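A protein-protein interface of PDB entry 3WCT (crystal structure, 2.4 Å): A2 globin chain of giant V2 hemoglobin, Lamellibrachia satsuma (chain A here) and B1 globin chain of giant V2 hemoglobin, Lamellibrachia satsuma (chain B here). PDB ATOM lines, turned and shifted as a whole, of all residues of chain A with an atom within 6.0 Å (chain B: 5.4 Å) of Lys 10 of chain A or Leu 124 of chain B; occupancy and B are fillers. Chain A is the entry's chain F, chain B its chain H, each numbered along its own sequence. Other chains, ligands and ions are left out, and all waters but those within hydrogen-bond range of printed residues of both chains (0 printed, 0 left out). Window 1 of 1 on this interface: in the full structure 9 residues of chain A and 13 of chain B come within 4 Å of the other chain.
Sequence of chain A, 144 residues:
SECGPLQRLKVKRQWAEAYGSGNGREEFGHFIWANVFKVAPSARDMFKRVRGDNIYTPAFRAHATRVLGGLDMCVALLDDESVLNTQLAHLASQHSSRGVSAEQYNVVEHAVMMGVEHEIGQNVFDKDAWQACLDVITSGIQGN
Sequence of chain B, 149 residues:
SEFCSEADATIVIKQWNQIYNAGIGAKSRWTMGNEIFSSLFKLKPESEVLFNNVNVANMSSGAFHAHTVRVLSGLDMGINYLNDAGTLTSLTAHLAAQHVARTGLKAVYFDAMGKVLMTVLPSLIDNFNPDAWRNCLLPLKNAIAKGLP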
ATOM      1  N   PRO A   5       2.964  -2.354  17.351  1.00  0.00           N
ATOM      2  CA  PRO A   5       3.116  -0.920  17.644  1.00  0.00           C
ATOM      3  C   PRO A   5       4.570  -0.455  17.735  1.00  0.00           C
ATOM      4  O   PRO A   5       4.905   0.628  17.261  1.00  0.00           O
ATOM      5  CB  PRO A   5       2.391  -0.758  18.976  1.00  0.00           C
ATOM      6  CG  PRO A   5       1.340  -1.843  18.927  1.00  0.00           C
ATOM      7  CD  PRO A   5       2.106  -3.005  18.358  1.00  0.00           C
ATOM      8  N   LEU A   6       5.423  -1.281  18.339  1.00  0.00           N
ATOM      9  CA  LEU A   6       6.843  -0.953  18.508  1.00  0.00           C
ATOM     10  C   LEU A   6       7.623  -1.004  17.199  1.00  0.00           C
ATOM     11  O   LEU A   6       8.478  -0.161  16.955  1.00  0.00           O
ATOM     12  CB  LEU A   6       7.491  -1.897  19.526  1.00  0.00           C
ATOM     13  CG  LEU A   6       6.839  -1.951  20.909  1.00  0.00           C
ATOM     14  CD1 LEU A   6       7.607  -2.931  21.790  1.00  0.00           C
ATOM     15  CD2 LEU A   6       6.819  -0.571  21.547  1.00  0.00           C
ATOM     16  N   GLN A   7       7.346  -1.994  16.360  1.00  0.00           N
ATOM     17  CA  GLN A   7       8.035  -2.085  15.077  1.00  0.00           C
ATOM     18  C   GLN A   7       7.645  -0.896  14.193  1.00  0.00           C
ATOM     19  O   GLN A   7       8.429  -0.440  13.359  1.00  0.00           O
ATOM     20  CB  GLN A   7       7.671  -3.380  14.358  1.00  0.00           C
ATOM     21  CG  GLN A   7       8.218  -4.645  14.993  1.00  0.00           C
ATOM     22  CD  GLN A   7       7.547  -4.986  16.307  1.00  0.00           C
ATOM     23  OE1 GLN A   7       6.332  -4.822  16.462  1.00  0.00           O
ATOM     24  NE2 GLN A   7       8.332  -5.492  17.256  1.00  0.00           N
ATOM     25  N   ARG A   8       6.427  -0.391  14.377  1.00  0.00           N
ATOM     26  CA  ARG A   8       5.959   0.743  13.583  1.00  0.00           C
ATOM     27  C   ARG A   8       6.635   2.036  14.008  1.00  0.00           C
ATOM     28  O   ARG A   8       6.876   2.911  13.173  1.00  0.00           O
ATOM     29  CB  ARG A   8       4.434   0.876  13.696  1.00  0.00           C
ATOM     30  CG  ARG A   8       3.703  -0.311  13.098  1.00  0.00           C
ATOM     31  CD  ARG A   8       2.213  -0.281  13.363  1.00  0.00           C
ATOM     32  NE  ARG A   8       1.621  -1.518  12.871  1.00  0.00           N
ATOM     33  CZ  ARG A   8       0.743  -1.596  11.879  1.00  0.00           C
ATOM     34  NH1 ARG A   8       0.324  -0.499  11.261  1.00  0.00           N
ATOM     35  NH2 ARG A   8       0.311  -2.786  11.485  1.00  0.00           N
ATOM     36  N   LEU A   9       6.926   2.159  15.302  1.00  0.00           N
ATOM     37  CA  LEU A   9       7.605   3.348  15.798  1.00  0.00           C
ATOM     38  C   LEU A   9       9.055   3.337  15.309  1.00  0.00           C
ATOM     39  O   LEU A   9       9.589   4.363  14.933  1.00  0.00           O
ATOM     40  CB  LEU A   9       7.589   3.403  17.328  1.00  0.00           C
ATOM     41  CG  LEU A   9       6.287   3.833  18.015  1.00  0.00           C
ATOM     42  CD1 LEU A   9       6.528   3.921  19.530  1.00  0.00           C
ATOM     43  CD2 LEU A   9       5.817   5.187  17.485  1.00  0.00           C
ATOM     44  N   LYS A  10       9.672   2.162  15.325  1.00  0.00           N
ATOM     45  CA  LYS A  10      11.051   1.971  14.882  1.00  0.00           C
ATOM     46  C   LYS A  10      11.165   2.340  13.401  1.00  0.00           C
ATOM     47  O   LYS A  10      12.006   3.151  12.997  1.00  0.00           O
ATOM     48  CB  LYS A  10      11.445   0.499  15.046  1.00  0.00           C
ATOM     49  CG  LYS A  10      12.932   0.199  14.970  1.00  0.00           C
ATOM     50  CD  LYS A  10      13.621   0.625  16.261  1.00  0.00           C
ATOM     51  CE  LYS A  10      15.082   0.190  16.311  1.00  0.00           C
ATOM     52  NZ  LYS A  10      15.264  -1.272  16.557  1.00  0.00           N
ATOM     53  N   VAL A  11      10.306   1.717  12.605  1.00  0.00           N
ATOM     54  CA  VAL A  11      10.280   1.933  11.170  1.00  0.00           C
ATOM     55  C   VAL A  11      10.060   3.394  10.854  1.00  0.00           C
ATOM     56  O   VAL A  11      10.647   3.908   9.901  1.00  0.00           O
ATOM     57  CB  VAL A  11       9.184   1.075  10.492  1.00  0.00           C
ATOM     58  CG1 VAL A  11       8.988   1.493   9.038  1.00  0.00           C
ATOM     59  CG2 VAL A  11       9.578  -0.390  10.562  1.00  0.00           C
ATOM     60  N   LYS A  12       9.230   4.066  11.652  1.00  0.00           N
ATOM     61  CA  LYS A  12       8.975   5.492  11.441  1.00  0.00           C
ATOM     62  C   LYS A  12      10.253   6.290  11.623  1.00  0.00           C
ATOM     63  O   LYS A  12      10.605   7.127  10.786  1.00  0.00           O
ATOM     64  CB  LYS A  12       7.947   6.033  12.442  1.00  0.00           C
ATOM     65  CG  LYS A  12       6.503   5.730  12.126  1.00  0.00           C
ATOM     66  CD  LYS A  12       5.613   6.259  13.250  1.00  0.00           C
ATOM     67  CE  LYS A  12       4.137   6.092  12.929  1.00  0.00           C
ATOM     68  NZ  LYS A  12       3.667   7.025  11.861  1.00  0.00           N
ATOM     69  N   ARG A  13      10.931   6.038  12.742  1.00  0.00           N
ATOM     70  CA  ARG A  13      12.156   6.752  13.044  1.00  0.00           C
ATOM     71  C   ARG A  13      13.261   6.468  12.029  1.00  0.00           C
ATOM     72  O   ARG A  13      13.811   7.395  11.453  1.00  0.00           O
ATOM     73  CB  ARG A  13      12.647   6.425  14.466  1.00  0.00           C
ATOM     74  CG  ARG A  13      13.758   7.366  14.958  1.00  0.00           C
ATOM     75  CD  ARG A  13      14.000   7.218  16.456  1.00  0.00           C
ATOM     76  NE  ARG A  13      14.218   5.824  16.841  1.00  0.00           N
ATOM     77  CZ  ARG A  13      15.307   5.130  16.541  1.00  0.00           C
ATOM     78  NH1 ARG A  13      15.405   3.860  16.935  1.00  0.00           N
ATOM     79  NH2 ARG A  13      16.306   5.710  15.865  1.00  0.00           N
ATOM     80  N   GLN A  14      13.579   5.202  11.792  1.00  0.00           N
ATOM     81  CA  GLN A  14      14.649   4.902  10.856  1.00  0.00           C
ATOM     82  C   GLN A  14      14.290   5.453   9.485  1.00  0.00           C
ATOM     83  O   GLN A  14      15.138   6.024   8.802  1.00  0.00           O
ATOM     84  CB  GLN A  14      14.941   3.391  10.820  1.00  0.00           C
ATOM     85  CG  GLN A  14      15.291   2.831  12.194  1.00  0.00           C
ATOM     86  CD  GLN A  14      16.047   1.503  12.142  1.00  0.00           C
ATOM     87  OE1 GLN A  14      15.811   0.669  11.267  1.00  0.00           O
ATOM     88  NE2 GLN A  14      16.958   1.298  13.106  1.00  0.00           N
ATOM     89  N   TRP A  15      13.026   5.325   9.092  1.00  0.00           N
ATOM     90  CA  TRP A  15      12.612   5.866   7.798  1.00  0.00           C
ATOM     91  C   TRP A  15      12.900   7.372   7.721  1.00  0.00           C
ATOM     92  O   TRP A  15      13.402   7.871   6.706  1.00  0.00           O
ATOM     93  CB  TRP A  15      11.123   5.613   7.542  1.00  0.00           C
ATOM     94  CG  TRP A  15      10.606   6.405   6.387  1.00  0.00           C
ATOM     95  CD1 TRP A  15       9.898   7.562   6.452  1.00  0.00           C
ATOM     96  CD2 TRP A  15      10.849   6.157   4.995  1.00  0.00           C
ATOM     97  NE1 TRP A  15       9.685   8.058   5.186  1.00  0.00           N
ATOM     98  CE2 TRP A  15      10.257   7.214   4.273  1.00  0.00           C
ATOM     99  CE3 TRP A  15      11.512   5.144   4.290  1.00  0.00           C
ATOM    100  CZ2 TRP A  15      10.305   7.297   2.873  1.00  0.00           C
ATOM    101  CZ3 TRP A  15      11.565   5.224   2.890  1.00  0.00           C
ATOM    102  CH2 TRP A  15      10.961   6.296   2.200  1.00  0.00           C
ATOM    103  N   VAL A 124      22.547  -0.539  13.017  1.00  0.00           N
ATOM    104  CA  VAL A 124      21.307  -0.105  13.655  1.00  0.00           C
ATOM    105  C   VAL A 124      20.075  -0.578  12.893  1.00  0.00           C
ATOM    106  O   VAL A 124      18.972  -0.601  13.433  1.00  0.00           O
ATOM    107  CB  VAL A 124      21.239   1.440  13.787  1.00  0.00           C
ATOM    108  CG1 VAL A 124      22.363   1.941  14.682  1.00  0.00           C
ATOM    109  CG2 VAL A 124      21.312   2.090  12.409  1.00  0.00           C
ATOM    110  N   ASP A 126      17.048  -2.318  11.652  1.00  0.00           N
ATOM    111  CA  ASP A 126      16.199  -3.327  12.286  1.00  0.00           C
ATOM    112  C   ASP A 126      15.438  -4.069  11.215  1.00  0.00           C
ATOM    113  O   ASP A 126      14.338  -3.676  10.857  1.00  0.00           O
ATOM    114  CB  ASP A 126      15.224  -2.669  13.262  1.00  0.00           C
ATOM    115  CG  ASP A 126      14.466  -3.681  14.104  1.00  0.00           C
ATOM    116  OD1 ASP A 126      13.998  -3.308  15.199  1.00  0.00           O
ATOM    117  OD2 ASP A 126      14.327  -4.840  13.675  1.00  0.00           O
ATOM    118  N   ALA A 129      11.700  -5.569  12.000  1.00  0.00           N
ATOM    119  CA  ALA A 129      10.658  -4.546  12.011  1.00  0.00           C
ATOM    120  C   ALA A 129      10.374  -4.019  10.601  1.00  0.00           C
ATOM    121  O   ALA A 129       9.224  -3.742  10.263  1.00  0.00           O
ATOM    122  CB  ALA A 129      11.055  -3.409  12.916  1.00  0.00           C
ATOM    123  N   TRP A 130      11.415  -3.885   9.780  1.00  0.00           N
ATOM    124  CA  TRP A 130      11.239  -3.393   8.411  1.00  0.00           C
ATOM    125  C   TRP A 130      10.555  -4.382   7.479  1.00  0.00           C
ATOM    126  O   TRP A 130       9.732  -3.992   6.658  1.00  0.00           O
ATOM    127  CB  TRP A 130      12.579  -2.978   7.787  1.00  0.00           C
ATOM    128  CG  TRP A 130      12.935  -1.565   8.096  1.00  0.00           C
ATOM    129  CD1 TRP A 130      13.680  -1.109   9.152  1.00  0.00           C
ATOM    130  CD2 TRP A 130      12.507  -0.410   7.378  1.00  0.00           C
ATOM    131  NE1 TRP A 130      13.733   0.261   9.133  1.00  0.00           N
ATOM    132  CE2 TRP A 130      13.018   0.716   8.054  1.00  0.00           C
ATOM    133  CE3 TRP A 130      11.730  -0.213   6.224  1.00  0.00           C
ATOM    134  CZ2 TRP A 130      12.789   2.023   7.610  1.00  0.00           C
ATOM    135  CZ3 TRP A 130      11.504   1.090   5.787  1.00  0.00           C
ATOM    136  CH2 TRP A 130      12.029   2.188   6.483  1.00  0.00           C
ATOM    137  N   GLN B  18      16.920   8.986  21.718  1.00  0.00           N
ATOM    138  CA  GLN B  18      16.547   8.557  20.372  1.00  0.00           C
ATOM    139  C   GLN B  18      15.036   8.419  20.249  1.00  0.00           C
ATOM    140  O   GLN B  18      14.445   8.796  19.244  1.00  0.00           O
ATOM    141  CB  GLN B  18      17.120   7.173  20.063  1.00  0.00           C
ATOM    142  CG  GLN B  18      18.601   7.062  19.746  1.00  0.00           C
ATOM    143  CD  GLN B  18      19.008   5.600  19.567  1.00  0.00           C
ATOM    144  OE1 GLN B  18      18.295   4.826  18.931  1.00  0.00           O
ATOM    145  NE2 GLN B  18      20.155   5.222  20.126  1.00  0.00           N
ATOM    146  N   ILE B  19      14.414   7.851  21.277  1.00  0.00           N
ATOM    147  CA  ILE B  19      12.979   7.613  21.241  1.00  0.00           C
ATOM    148  C   ILE B  19      12.133   8.545  22.108  1.00  0.00           C
ATOM    149  O   ILE B  19      10.900   8.524  22.026  1.00  0.00           O
ATOM    150  CB  ILE B  19      12.671   6.151  21.652  1.00  0.00           C
ATOM    151  CG1 ILE B  19      13.217   5.885  23.061  1.00  0.00           C
ATOM    152  CG2 ILE B  19      13.308   5.181  20.660  1.00  0.00           C
ATOM    153  CD1 ILE B  19      12.859   4.520  23.614  1.00  0.00           C
ATOM    154  N   MET B  32       4.157   3.718  23.555  1.00  0.00           N
ATOM    155  CA  MET B  32       5.200   2.954  24.240  1.00  0.00           C
ATOM    156  C   MET B  32       4.656   2.631  25.631  1.00  0.00           C
ATOM    157  O   MET B  32       4.901   1.557  26.187  1.00  0.00           O
ATOM    158  CB  MET B  32       6.475   3.780  24.381  1.00  0.00           C
ATOM    159  CG  MET B  32       7.170   4.112  23.076  1.00  0.00           C
ATOM    160  SD  MET B  32       8.403   5.398  23.350  1.00  0.00           S
ATOM    161  CE  MET B  32       9.683   4.469  24.064  1.00  0.00           C
ATOM    162  N   VAL B 120      11.171  -4.594  25.963  1.00  0.00           N
ATOM    163  CA  VAL B 120      10.554  -3.586  25.107  1.00  0.00           C
ATOM    164  C   VAL B 120      11.529  -2.639  24.375  1.00  0.00           C
ATOM    165  O   VAL B 120      11.434  -2.453  23.158  1.00  0.00           O
ATOM    166  CB  VAL B 120       9.582  -2.707  25.939  1.00  0.00           C
ATOM    167  CG1 VAL B 120       9.258  -1.422  25.188  1.00  0.00           C
ATOM    168  CG2 VAL B 120       8.315  -3.478  26.252  1.00  0.00           C
ATOM    169  N   LEU B 121      12.455  -2.035  25.115  1.00  0.00           N
ATOM    170  CA  LEU B 121      13.393  -1.079  24.533  1.00  0.00           C
ATOM    171  C   LEU B 121      14.204  -1.552  23.328  1.00  0.00           C
ATOM    172  O   LEU B 121      14.320  -0.832  22.344  1.00  0.00           O
ATOM    173  CB  LEU B 121      14.314  -0.534  25.620  1.00  0.00           C
ATOM    174  CG  LEU B 121      13.541   0.238  26.695  1.00  0.00           C
ATOM    175  CD1 LEU B 121      14.483   0.671  27.803  1.00  0.00           C
ATOM    176  CD2 LEU B 121      12.855   1.448  26.073  1.00  0.00           C
ATOM    177  N   PRO B 122      14.774  -2.766  23.375  1.00  0.00           N
ATOM    178  CA  PRO B 122      15.533  -3.159  22.185  1.00  0.00           C
ATOM    179  C   PRO B 122      14.733  -3.083  20.882  1.00  0.00           C
ATOM    180  O   PRO B 122      15.318  -3.009  19.799  1.00  0.00           O
ATOM    181  CB  PRO B 122      16.010  -4.578  22.514  1.00  0.00           C
ATOM    182  CG  PRO B 122      15.161  -5.005  23.665  1.00  0.00           C
ATOM    183  CD  PRO B 122      14.913  -3.758  24.447  1.00  0.00           C
ATOM    184  N   SER B 123      13.404  -3.096  20.985  1.00  0.00           N
ATOM    185  CA  SER B 123      12.554  -3.014  19.800  1.00  0.00           C
ATOM    186  C   SER B 123      12.298  -1.560  19.391  1.00  0.00           C
ATOM    187  O   SER B 123      11.697  -1.296  18.352  1.00  0.00           O
ATOM    188  CB  SER B 123      11.207  -3.714  20.048  1.00  0.00           C
ATOM    189  OG  SER B 123      11.382  -5.107  20.263  1.00  0.00           O
ATOM    190  N   LEU B 124      12.747  -0.617  20.213  1.00  0.00           N
ATOM    191  CA  LEU B 124      12.559   0.797  19.910  1.00  0.00           C
ATOM    192  C   LEU B 124      13.874   1.493  19.621  1.00  0.00           C
ATOM    193  O   LEU B 124      13.960   2.330  18.729  1.00  0.00           O
ATOM    194  CB  LEU B 124      11.888   1.512  21.082  1.00  0.00           C
ATOM    195  CG  LEU B 124      10.454   1.088  21.402  1.00  0.00           C
ATOM    196  CD1 LEU B 124      10.052   1.560  22.789  1.00  0.00           C
ATOM    197  CD2 LEU B 124       9.526   1.645  20.335  1.00  0.00           C
ATOM    198  N   ILE B 125      14.893   1.120  20.388  1.00  0.00           N
ATOM    199  CA  ILE B 125      16.216   1.712  20.322  1.00  0.00           C
ATOM    200  C   ILE B 125      17.204   1.064  19.355  1.00  0.00           C
ATOM    201  O   ILE B 125      17.302  -0.164  19.264  1.00  0.00           O
ATOM    202  CB  ILE B 125      16.823   1.725  21.752  1.00  0.00           C
ATOM    203  CG1 ILE B 125      16.019   2.692  22.628  1.00  0.00           C
ATOM    204  CG2 ILE B 125      18.294   2.103  21.723  1.00  0.00           C
ATOM    205  CD1 ILE B 125      16.257   2.538  24.122  1.00  0.00           C
ATOM    206  N   ASP B 126      17.939   1.909  18.642  1.00  0.00           N
ATOM    207  CA  ASP B 126      18.946   1.439  17.713  1.00  0.00           C
ATOM    208  C   ASP B 126      20.049   0.785  18.516  1.00  0.00           C
ATOM    209  O   ASP B 126      20.564   1.373  19.466  1.00  0.00           O
ATOM    210  CB  ASP B 126      19.549   2.599  16.914  1.00  0.00           C
ATOM    211  CG  ASP B 126      18.601   3.155  15.874  1.00  0.00           C
ATOM    212  OD1 ASP B 126      17.639   2.443  15.503  1.00  0.00           O
ATOM    213  OD2 ASP B 126      18.829   4.295  15.413  1.00  0.00           O
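Leu 6 of chain A touches Leu 124 of chain B. Met 32 of chain B touches Leu 9 of chain A. CD1 of Leu 9 of chain A touches CD2 of Leu 124 of chain B, at 3.8 Å. O of Pro 122 of chain B touches NZ of Lys 10 of chain A (3.7 Å). Ser 123 of chain B touches Lys 10 of chain A (O to CD, 3.4 Å). Leu 124 of chain B touches Lys 10 of chain A. Lys 10 of chain A touches Ile 125 of chain B (NZ to O, 3.6 Å). Arg 13 of chain A touches Gln 18 of chain B (CD to O, 3.2 Å). Arg 13 of chain A touches Ile 19 of chain B (NE to CG2, 3.98 Å). Asp 126 of chain B touches Val 124 of chain A.
The side-chain carboxylate (OD1) of Asp 126 of chain A lies within salt-bridge range of the side-chain amino group (NZ) of Lys 10 of chain A (2.8 Å). The side-chain amide nitrogen (NE2) of Gln 14 of chain A is in hydrogen-bond range of the backbone carbonyl oxygen (O) of Val 124 of chain A, 2.8 Å away. The side-chain amide oxygen (OE1) of Gln 14 of chain A is in hydrogen-bond range of the backbone NH (N) of Asp 126 of chain A, 3.3 Å away. OE1 of Gln 14 of chain A lies within hydrogen-bond range of NE1 of Trp 130 of chain A, at 3.0 Å. The backbone NH of Asp 126 of chain B lies within hydrogen-bond range of the side-chain amide oxygen of Gln 18 of chain B.
The guanidinium group (NH1) of Arg 13 of chain A is in hydrogen-bond range of the backbone carbonyl oxygen (O) of Leu 124 of chain B, 2.8 Å away. NH2 of Arg 13 of chain A is in salt-bridge range of OD2 of Asp 126 of chain B, at 2.9 Å. NE2 of Gln 14 of chain A lies within hydrogen-bond range of OD1 of Asp 126 of chain B, at 2.7 Å.
Of chain A, only Leu 6 (3.7 Å), Leu 9 (3.8 Å), Lys 10 (3.0 Å) and Arg 13 (2.8 Å) come within 4 Å of Leu 124 of chain B. Printed residues of chain A within 4 Å of Pro 122 of chain B: Lys 10. Of the printed residues of chain B, Gln 14 of chain A touches Asp 126 (2.7 Å). Pro 5 of chain A touches none of the printed residues of chain B. Arg 8 of chain A touches none of the printed residues of chain B. The nearest printed residue of chain B that does not touch Lys 10 of chain A is Leu 121 of chain B (5.9 Å). The nearest printed residue of chain A that does not touch Ile 125 of chain B is Arg 13 of chain A (4.1 Å).
Of the 15 printed residues of chain A, 6 touch a printed residue of chain B. Hydrophobic or aromatic side chains of chain A that line the printed part of chain B: Leu 6, Leu 9 and Val 124. Of the 10 printed residues of chain B, 8 touch a printed residue of chain A. Printed residues of chain B that touch a printed residue of chain A: Gln 18, Ile 19, Met 32, Pro 122, Ser 123, Leu 124, Ile 125 and Asp 126. Hydrophobic or aromatic side chains of chain B that line the printed part of chain A: Ile 19, Met 32 and Leu 124.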
